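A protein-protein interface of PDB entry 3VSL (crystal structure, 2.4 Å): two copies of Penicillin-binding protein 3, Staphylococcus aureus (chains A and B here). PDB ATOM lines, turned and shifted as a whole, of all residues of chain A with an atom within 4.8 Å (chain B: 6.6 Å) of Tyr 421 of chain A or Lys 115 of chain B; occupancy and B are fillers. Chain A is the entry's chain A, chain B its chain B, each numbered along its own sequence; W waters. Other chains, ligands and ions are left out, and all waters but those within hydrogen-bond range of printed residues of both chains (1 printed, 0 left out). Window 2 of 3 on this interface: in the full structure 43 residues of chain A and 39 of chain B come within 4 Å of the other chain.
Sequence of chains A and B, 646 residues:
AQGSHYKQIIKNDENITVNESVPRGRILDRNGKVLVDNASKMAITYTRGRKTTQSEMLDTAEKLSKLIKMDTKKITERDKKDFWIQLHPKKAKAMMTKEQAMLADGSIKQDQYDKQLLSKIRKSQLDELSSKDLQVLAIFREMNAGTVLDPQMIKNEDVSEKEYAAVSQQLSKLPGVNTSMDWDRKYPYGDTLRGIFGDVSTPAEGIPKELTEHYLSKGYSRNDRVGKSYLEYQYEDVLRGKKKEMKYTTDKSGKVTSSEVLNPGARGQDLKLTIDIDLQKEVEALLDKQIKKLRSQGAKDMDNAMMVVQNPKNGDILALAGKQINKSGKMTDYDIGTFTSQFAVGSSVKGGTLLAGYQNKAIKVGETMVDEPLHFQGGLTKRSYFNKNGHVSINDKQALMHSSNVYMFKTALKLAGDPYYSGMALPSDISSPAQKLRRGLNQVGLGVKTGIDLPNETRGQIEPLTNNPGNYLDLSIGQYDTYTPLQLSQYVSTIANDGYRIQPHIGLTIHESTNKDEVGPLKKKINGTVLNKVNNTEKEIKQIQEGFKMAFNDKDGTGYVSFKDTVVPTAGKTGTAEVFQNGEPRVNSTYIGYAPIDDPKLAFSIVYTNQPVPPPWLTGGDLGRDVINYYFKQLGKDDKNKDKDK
The side-chain hydroxyl of Tyr 421 of chain A sits close to the side-chain amino group of Lys 81 of chain B.
The backbone carbonyl oxygen of Pro 419 of chain A sits at hydrogen-bond distance from the guanidinium group of Arg 78 of chain B, at 2.4 Å.
NE of Arg 78 of chain B lies within salt-bridge range of OD1 of Asp 418 of chain A, 3.5 Å away.
NZ of Lys 81 of chain B lies within hydrogen-bond range of O of Ile 121 of chain B (3.0 Å).
The side-chain hydroxyl (OG) of Ser 119 of chain B lies within hydrogen-bond range of the backbone carbonyl oxygen (O) of Lys 115 of chain B (3.0 Å).
The side-chain sulfur (SD) of Met 424 of chain A sits at hydrogen-bond distance from the backbone NH (N) of Tyr 421 of chain A (3.5 Å).
The backbone carbonyl oxygen of Gln 116 of chain B lies within hydrogen-bond range of the side-chain hydroxyl of Ser 119 of chain B.
The side-chain amino group of Lys 115 of chain B is in salt-bridge range of the side-chain carboxylate of Asp 111 of chain B (2.7 Å).
The side-chain carboxylate (OE2) of Glu 77 of chain B lies within salt-bridge range of the side-chain amino group (NZ) of Lys 81 of chain B (3.5 Å).
Tyr 420 of chain A touches Lys 115 of chain B (O to CE, 3.9 Å).
Arg 78 of chain B touches Tyr 421 of chain A.
Tyr 421 of chain A touches Lys 115 of chain B.
CD2 of Tyr 421 of chain A touches CD2 of Leu 118 of chain B, at 3.4 Å.
O of Ser 422 of chain A touches OG of Ser 119 of chain B, 3.7 Å away.
Tyr 421 of chain A touches just these residues of chain B: Arg 78 (3.3 Å), Lys 81 (3.2 Å), Lys 115 (3.6 Å) and Leu 118 (3.4 Å).
Lys 115 of chain B touches two residues of chain A.
Of the printed residues of chain B, Tyr 420 of chain A touches Lys 115 (3.9 Å).
Printed residues of chain B within 4 Å of Asp 418 of chain A: Arg 78.
Of the printed residues of chain B, Pro 419 of chain A touches Arg 78.
Met 424 of chain A touches none of the printed residues of chain B.
The nearest printed residue of chain B that does not touch Tyr 421 of chain A is Ser 119 of chain B (4.1 Å).
The nearest residue of chain A that does not touch Lys 115 of chain B is Met 369 of chain A (4.2 Å).
The nearest printed residue of chain A that does not touch Leu 118 of chain B is Pro 419 of chain A (5.8 Å).
Of the 9 printed residues of chain A, 5 touch a printed residue of chain B.
Among the printed residues, 8 pairs touch across the chains.
No position is printed for both chains.
Of the 8 pairs that touch across the chains among the printed residues, none has its exchanged pair printed and touching as well.
Water W1 lies within hydrogen-bond range of NH2 of Arg 78 of chain B, O of Tyr 420 of chain A and O of Pro 419 of chain A.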
ATOM      1  N   MET A 369     -14.012  18.641   9.970  1.00  0.00           N
ATOM      2  CA  MET A 369     -12.856  17.905   9.418  1.00  0.00           C
ATOM      3  C   MET A 369     -12.363  16.734  10.258  1.00  0.00           C
ATOM      4  O   MET A 369     -12.758  16.570  11.408  1.00  0.00           O
ATOM      5  CB  MET A 369     -11.696  18.837   9.040  1.00  0.00           C
ATOM      6  CG  MET A 369     -11.096  18.627   7.622  1.00  0.00           C
ATOM      7  SD  MET A 369     -10.198  17.076   7.284  1.00  0.00           S
ATOM      8  CE  MET A 369      -8.505  17.519   7.664  1.00  0.00           C
ATOM      9  N   HIS A 375       1.879  14.083  11.105  1.00  0.00           N
ATOM     10  CA  HIS A 375       3.287  13.812  10.785  1.00  0.00           C
ATOM     11  C   HIS A 375       4.062  14.964  10.153  1.00  0.00           C
ATOM     12  O   HIS A 375       3.651  15.531   9.143  1.00  0.00           O
ATOM     13  CB  HIS A 375       3.422  12.545   9.936  1.00  0.00           C
ATOM     14  CG  HIS A 375       2.947  11.313  10.631  1.00  0.00           C
ATOM     15  ND1 HIS A 375       1.705  10.754  10.395  1.00  0.00           N
ATOM     16  CD2 HIS A 375       3.527  10.538  11.576  1.00  0.00           C
ATOM     17  CE1 HIS A 375       1.553   9.688  11.155  1.00  0.00           C
ATOM     18  NE2 HIS A 375       2.648   9.531  11.880  1.00  0.00           N
ATOM     19  N   ASP A 418      -1.618  27.488   6.664  1.00  0.00           N
ATOM     20  CA  ASP A 418      -0.783  26.325   6.373  1.00  0.00           C
ATOM     21  C   ASP A 418      -1.473  25.023   6.752  1.00  0.00           C
ATOM     22  O   ASP A 418      -0.969  24.277   7.581  1.00  0.00           O
ATOM     23  CB  ASP A 418       0.520  26.468   7.165  1.00  0.00           C
ATOM     24  CG  ASP A 418       1.615  25.573   6.660  1.00  0.00           C
ATOM     25  OD1 ASP A 418       1.549  25.138   5.489  1.00  0.00           O
ATOM     26  OD2 ASP A 418       2.553  25.310   7.439  1.00  0.00           O
ATOM     27  N   PRO A 419      -2.631  24.743   6.146  1.00  0.00           N
ATOM     28  CA  PRO A 419      -3.434  23.599   6.603  1.00  0.00           C
ATOM     29  C   PRO A 419      -2.654  22.292   6.536  1.00  0.00           C
ATOM     30  O   PRO A 419      -1.724  22.172   5.741  1.00  0.00           O
ATOM     31  CB  PRO A 419      -4.603  23.567   5.613  1.00  0.00           C
ATOM     32  CG  PRO A 419      -4.598  24.931   4.977  1.00  0.00           C
ATOM     33  CD  PRO A 419      -3.177  25.346   4.925  1.00  0.00           C
ATOM     34  N   TYR A 420      -3.019  21.329   7.372  1.00  0.00           N
ATOM     35  CA  TYR A 420      -2.244  20.099   7.489  1.00  0.00           C
ATOM     36  C   TYR A 420      -2.191  19.281   6.213  1.00  0.00           C
ATOM     37  O   TYR A 420      -3.201  19.107   5.520  1.00  0.00           O
ATOM     38  CB  TYR A 420      -2.802  19.210   8.598  1.00  0.00           C
ATOM     39  CG  TYR A 420      -2.104  17.863   8.711  1.00  0.00           C
ATOM     40  CD1 TYR A 420      -0.876  17.756   9.349  1.00  0.00           C
ATOM     41  CD2 TYR A 420      -2.681  16.699   8.202  1.00  0.00           C
ATOM     42  CE1 TYR A 420      -0.236  16.532   9.475  1.00  0.00           C
ATOM     43  CE2 TYR A 420      -2.046  15.473   8.318  1.00  0.00           C
ATOM     44  CZ  TYR A 420      -0.818  15.395   8.956  1.00  0.00           C
ATOM     45  OH  TYR A 420      -0.165  14.184   9.084  1.00  0.00           O
ATOM     46  N   TYR A 421      -0.991  18.794   5.918  1.00  0.00           N
ATOM     47  CA  TYR A 421      -0.787  17.655   5.039  1.00  0.00           C
ATOM     48  C   TYR A 421       0.340  16.824   5.648  1.00  0.00           C
ATOM     49  O   TYR A 421       1.275  17.390   6.226  1.00  0.00           O
ATOM     50  CB  TYR A 421      -0.500  18.081   3.592  1.00  0.00           C
ATOM     51  CG  TYR A 421       0.714  18.956   3.324  1.00  0.00           C
ATOM     52  CD1 TYR A 421       1.979  18.406   3.123  1.00  0.00           C
ATOM     53  CD2 TYR A 421       0.578  20.333   3.199  1.00  0.00           C
ATOM     54  CE1 TYR A 421       3.083  19.215   2.834  1.00  0.00           C
ATOM     55  CE2 TYR A 421       1.675  21.150   2.911  1.00  0.00           C
ATOM     56  CZ  TYR A 421       2.921  20.588   2.732  1.00  0.00           C
ATOM     57  OH  TYR A 421       4.000  21.405   2.461  1.00  0.00           O
ATOM     58  N   SER A 422       0.237  15.497   5.569  1.00  0.00           N
ATOM     59  CA  SER A 422       1.260  14.644   6.168  1.00  0.00           C
ATOM     60  C   SER A 422       2.644  14.954   5.612  1.00  0.00           C
ATOM     61  O   SER A 422       2.814  15.141   4.411  1.00  0.00           O
ATOM     62  CB  SER A 422       0.948  13.163   5.992  1.00  0.00           C
ATOM     63  OG  SER A 422       1.985  12.394   6.559  1.00  0.00           O
ATOM     64  N   GLY A 423       3.628  15.024   6.500  1.00  0.00           N
ATOM     65  CA  GLY A 423       4.998  15.299   6.107  1.00  0.00           C
ATOM     66  C   GLY A 423       5.265  16.738   5.701  1.00  0.00           C
ATOM     67  O   GLY A 423       6.206  17.009   4.951  1.00  0.00           O
ATOM     68  N   MET A 424       4.442  17.664   6.186  1.00  0.00           N
ATOM     69  CA  MET A 424       4.672  19.080   5.940  1.00  0.00           C
ATOM     70  C   MET A 424       5.753  19.541   6.902  1.00  0.00           C
ATOM     71  O   MET A 424       5.902  18.966   7.973  1.00  0.00           O
ATOM     72  CB  MET A 424       3.379  19.873   6.187  1.00  0.00           C
ATOM     73  CG  MET A 424       3.025  20.050   7.662  1.00  0.00           C
ATOM     74  SD  MET A 424       1.282  20.409   8.033  1.00  0.00           S
ATOM     75  CE  MET A 424       1.087  21.895   7.032  1.00  0.00           C
ATOM     76  N   GLU B  77       6.484  29.029   2.732  1.00  0.00           N
ATOM     77  CA  GLU B  77       6.790  27.909   1.850  1.00  0.00           C
ATOM     78  C   GLU B  77       5.507  27.400   1.210  1.00  0.00           C
ATOM     79  O   GLU B  77       5.494  27.059   0.028  1.00  0.00           O
ATOM     80  CB  GLU B  77       7.476  26.788   2.645  1.00  0.00           C
ATOM     81  CG  GLU B  77       8.043  25.638   1.826  1.00  0.00           C
ATOM     82  CD  GLU B  77       8.325  24.426   2.696  1.00  0.00           C
ATOM     83  OE1 GLU B  77       9.458  24.299   3.208  1.00  0.00           O
ATOM     84  OE2 GLU B  77       7.394  23.613   2.892  1.00  0.00           O
ATOM     85  N   ARG B  78       4.427  27.360   1.994  1.00  0.00           N
ATOM     86  CA  ARG B  78       3.135  26.910   1.480  1.00  0.00           C
ATOM     87  C   ARG B  78       2.612  27.846   0.396  1.00  0.00           C
ATOM     88  O   ARG B  78       2.177  27.380  -0.659  1.00  0.00           O
ATOM     89  CB  ARG B  78       2.100  26.757   2.581  1.00  0.00           C
ATOM     90  CG  ARG B  78       0.736  26.346   2.061  1.00  0.00           C
ATOM     91  CD  ARG B  78       0.735  24.904   1.580  1.00  0.00           C
ATOM     92  NE  ARG B  78       0.106  24.018   2.561  1.00  0.00           N
ATOM     93  CZ  ARG B  78      -1.153  23.601   2.491  1.00  0.00           C
ATOM     94  NH1 ARG B  78      -1.923  23.970   1.479  1.00  0.00           N
ATOM     95  NH2 ARG B  78      -1.633  22.806   3.423  1.00  0.00           N
ATOM     96  N   LYS B  81       4.213  26.855  -2.635  1.00  0.00           N
ATOM     97  CA  LYS B  81       3.837  25.569  -3.215  1.00  0.00           C
ATOM     98  C   LYS B  81       2.500  25.659  -3.924  1.00  0.00           C
ATOM     99  O   LYS B  81       2.359  25.187  -5.050  1.00  0.00           O
ATOM    100  CB  LYS B  81       3.876  24.453  -2.181  1.00  0.00           C
ATOM    101  CG  LYS B  81       5.292  23.922  -1.974  1.00  0.00           C
ATOM    102  CD  LYS B  81       5.586  23.510  -0.540  1.00  0.00           C
ATOM    103  CE  LYS B  81       5.380  22.027  -0.359  1.00  0.00           C
ATOM    104  NZ  LYS B  81       6.518  21.363   0.346  1.00  0.00           N
ATOM    105  N   MET B  96       2.548  13.315 -10.649  1.00  0.00           N
ATOM    106  CA  MET B  96       1.418  12.686  -9.987  1.00  0.00           C
ATOM    107  C   MET B  96       0.750  11.592 -10.810  1.00  0.00           C
ATOM    108  O   MET B  96      -0.423  11.306 -10.584  1.00  0.00           O
ATOM    109  CB  MET B  96       0.375  13.741  -9.631  1.00  0.00           C
ATOM    110  CG  MET B  96       0.852  14.800  -8.655  1.00  0.00           C
ATOM    111  SD  MET B  96       1.364  14.141  -7.058  1.00  0.00           S
ATOM    112  CE  MET B  96      -0.154  13.401  -6.469  1.00  0.00           C
ATOM    113  N   GLN B 110      -9.685  13.307  -4.193  1.00  0.00           N
ATOM    114  CA  GLN B 110      -9.015  14.583  -4.480  1.00  0.00           C
ATOM    115  C   GLN B 110      -8.217  15.187  -3.321  1.00  0.00           C
ATOM    116  O   GLN B 110      -7.142  15.726  -3.542  1.00  0.00           O
ATOM    117  CB  GLN B 110     -10.005  15.624  -4.997  1.00  0.00           C
ATOM    118  CG  GLN B 110      -9.339  16.816  -5.656  1.00  0.00           C
ATOM    119  CD  GLN B 110      -8.853  16.503  -7.056  1.00  0.00           C
ATOM    120  OE1 GLN B 110      -7.653  16.476  -7.317  1.00  0.00           O
ATOM    121  NE2 GLN B 110      -9.789  16.272  -7.969  1.00  0.00           N
ATOM    122  N   ASP B 111      -8.745  15.118  -2.099  1.00  0.00           N
ATOM    123  CA  ASP B 111      -8.029  15.656  -0.938  1.00  0.00           C
ATOM    124  C   ASP B 111      -6.695  14.966  -0.716  1.00  0.00           C
ATOM    125  O   ASP B 111      -5.686  15.641  -0.492  1.00  0.00           O
ATOM    126  CB  ASP B 111      -8.852  15.577   0.352  1.00  0.00           C
ATOM    127  CG  ASP B 111      -7.981  15.701   1.606  1.00  0.00           C
ATOM    128  OD1 ASP B 111      -7.451  16.812   1.863  1.00  0.00           O
ATOM    129  OD2 ASP B 111      -7.828  14.688   2.331  1.00  0.00           O
ATOM    130  N   GLN B 112      -6.700  13.632  -0.752  1.00  0.00           N
ATOM    131  CA  GLN B 112      -5.471  12.841  -0.680  1.00  0.00           C
ATOM    132  C   GLN B 112      -4.513  13.215  -1.822  1.00  0.00           C
ATOM    133  O   GLN B 112      -3.294  13.288  -1.638  1.00  0.00           O
ATOM    134  CB  GLN B 112      -5.793  11.347  -0.742  1.00  0.00           C
ATOM    135  CG  GLN B 112      -7.031  10.934   0.058  1.00  0.00           C
ATOM    136  CD  GLN B 112      -7.390   9.458  -0.116  1.00  0.00           C
ATOM    137  OE1 GLN B 112      -8.475   9.121  -0.597  1.00  0.00           O
ATOM    138  NE2 GLN B 112      -6.478   8.573   0.278  1.00  0.00           N
ATOM    139  N   TYR B 113      -5.083  13.455  -3.000  1.00  0.00           N
ATOM    140  CA  TYR B 113      -4.303  13.793  -4.182  1.00  0.00           C
ATOM    141  C   TYR B 113      -3.531  15.082  -3.932  1.00  0.00           C
ATOM    142  O   TYR B 113      -2.317  15.139  -4.141  1.00  0.00           O
ATOM    143  CB  TYR B 113      -5.219  13.928  -5.405  1.00  0.00           C
ATOM    144  CG  TYR B 113      -4.523  14.375  -6.664  1.00  0.00           C
ATOM    145  CD1 TYR B 113      -4.246  15.713  -6.890  1.00  0.00           C
ATOM    146  CD2 TYR B 113      -4.151  13.459  -7.636  1.00  0.00           C
ATOM    147  CE1 TYR B 113      -3.611  16.125  -8.034  1.00  0.00           C
ATOM    148  CE2 TYR B 113      -3.518  13.864  -8.793  1.00  0.00           C
ATOM    149  CZ  TYR B 113      -3.252  15.199  -8.985  1.00  0.00           C
ATOM    150  OH  TYR B 113      -2.622  15.608 -10.133  1.00  0.00           O
ATOM    151  N   ASP B 114      -4.253  16.109  -3.480  1.00  0.00           N
ATOM    152  CA  ASP B 114      -3.688  17.424  -3.210  1.00  0.00           C
ATOM    153  C   ASP B 114      -2.698  17.358  -2.062  1.00  0.00           C
ATOM    154  O   ASP B 114      -1.680  18.051  -2.060  1.00  0.00           O
ATOM    155  CB  ASP B 114      -4.805  18.416  -2.904  1.00  0.00           C
ATOM    156  CG  ASP B 114      -5.768  18.575  -4.061  1.00  0.00           C
ATOM    157  OD1 ASP B 114      -5.371  18.318  -5.217  1.00  0.00           O
ATOM    158  OD2 ASP B 114      -6.923  18.965  -3.817  1.00  0.00           O
ATOM    159  N   LYS B 115      -3.002  16.517  -1.085  1.00  0.00           N
ATOM    160  CA  LYS B 115      -2.094  16.289   0.028  1.00  0.00           C
ATOM    161  C   LYS B 115      -0.797  15.654  -0.437  1.00  0.00           C
ATOM    162  O   LYS B 115       0.264  16.018   0.052  1.00  0.00           O
ATOM    163  CB  LYS B 115      -2.737  15.404   1.109  1.00  0.00           C
ATOM    164  CG  LYS B 115      -3.220  16.145   2.330  1.00  0.00           C
ATOM    165  CD  LYS B 115      -4.630  15.736   2.667  1.00  0.00           C
ATOM    166  CE  LYS B 115      -4.940  15.920   4.136  1.00  0.00           C
ATOM    167  NZ  LYS B 115      -6.332  16.398   4.292  1.00  0.00           N
ATOM    168  N   GLN B 116      -0.870  14.708  -1.372  1.00  0.00           N
ATOM    169  CA  GLN B 116       0.351  14.039  -1.828  1.00  0.00           C
ATOM    170  C   GLN B 116       1.201  14.938  -2.717  1.00  0.00           C
ATOM    171  O   GLN B 116       2.423  14.971  -2.594  1.00  0.00           O
ATOM    172  CB  GLN B 116       0.053  12.698  -2.495  1.00  0.00           C
ATOM    173  CG  GLN B 116      -0.379  11.647  -1.495  1.00  0.00           C
ATOM    174  CD  GLN B 116      -0.214  10.256  -2.032  1.00  0.00           C
ATOM    175  OE1 GLN B 116       0.904   9.809  -2.298  1.00  0.00           O
ATOM    176  NE2 GLN B 116      -1.324   9.554  -2.205  1.00  0.00           N
ATOM    177  N   LEU B 117       0.544  15.688  -3.587  1.00  0.00           N
ATOM    178  CA  LEU B 117       1.205  16.699  -4.384  1.00  0.00           C
ATOM    179  C   LEU B 117       2.053  17.647  -3.538  1.00  0.00           C
ATOM    180  O   LEU B 117       3.214  17.895  -3.848  1.00  0.00           O
ATOM    181  CB  LEU B 117       0.146  17.503  -5.126  1.00  0.00           C
ATOM    182  CG  LEU B 117       0.445  17.967  -6.543  1.00  0.00           C
ATOM    183  CD1 LEU B 117      -0.447  19.150  -6.863  1.00  0.00           C
ATOM    184  CD2 LEU B 117       1.905  18.319  -6.739  1.00  0.00           C
ATOM    185  N   LEU B 118       1.459  18.194  -2.484  1.00  0.00           N
ATOM    186  CA  LEU B 118       2.170  19.091  -1.577  1.00  0.00           C
ATOM    187  C   LEU B 118       3.468  18.479  -0.999  1.00  0.00           C
ATOM    188  O   LEU B 118       4.472  19.179  -0.877  1.00  0.00           O
ATOM    189  CB  LEU B 118       1.233  19.603  -0.465  1.00  0.00           C
ATOM    190  CG  LEU B 118       0.728  21.058  -0.495  1.00  0.00           C
ATOM    191  CD1 LEU B 118       0.672  21.587  -1.905  1.00  0.00           C
ATOM    192  CD2 LEU B 118      -0.643  21.180   0.159  1.00  0.00           C
ATOM    193  N   SER B 119       3.468  17.186  -0.670  1.00  0.00           N
ATOM    194  CA  SER B 119       4.685  16.547  -0.147  1.00  0.00           C
ATOM    195  C   SER B 119       5.787  16.380  -1.199  1.00  0.00           C
ATOM    196  O   SER B 119       6.969  16.405  -0.862  1.00  0.00           O
ATOM    197  CB  SER B 119       4.397  15.188   0.489  1.00  0.00           C
ATOM    198  OG  SER B 119       3.019  14.987   0.711  1.00  0.00           O
ATOM    199  N   LYS B 120       5.398  16.208  -2.461  1.00  0.00           N
ATOM    200  CA  LYS B 120       6.333  15.933  -3.565  1.00  0.00           C
ATOM    201  C   LYS B 120       7.054  17.166  -4.100  1.00  0.00           C
ATOM    202  O   LYS B 120       8.151  17.062  -4.657  1.00  0.00           O
ATOM    203  CB  LYS B 120       5.597  15.267  -4.720  1.00  0.00           C
ATOM    204  CG  LYS B 120       5.647  13.785  -4.685  1.00  0.00           C
ATOM    205  CD  LYS B 120       4.403  13.223  -5.292  1.00  0.00           C
ATOM    206  CE  LYS B 120       4.592  11.759  -5.577  1.00  0.00           C
ATOM    207  NZ  LYS B 120       3.449  11.204  -6.333  1.00  0.00           N
ATOM    208  N   ILE B 121       6.411  18.321  -3.946  1.00  0.00           N
ATOM    209  CA  ILE B 121       6.996  19.609  -4.303  1.00  0.00           C
ATOM    210  C   ILE B 121       8.084  19.987  -3.291  1.00  0.00           C
ATOM    211  O   ILE B 121       7.767  20.296  -2.134  1.00  0.00           O
ATOM    212  CB  ILE B 121       5.920  20.721  -4.294  1.00  0.00           C
ATOM    213  CG1 ILE B 121       4.745  20.363  -5.207  1.00  0.00           C
ATOM    214  CG2 ILE B 121       6.511  22.053  -4.695  1.00  0.00           C
ATOM    215  CD1 ILE B 121       3.438  20.976  -4.741  1.00  0.00           C
HETATM  216  O   HOH W   1      -3.486  20.784   3.263  1.00  0.00           O
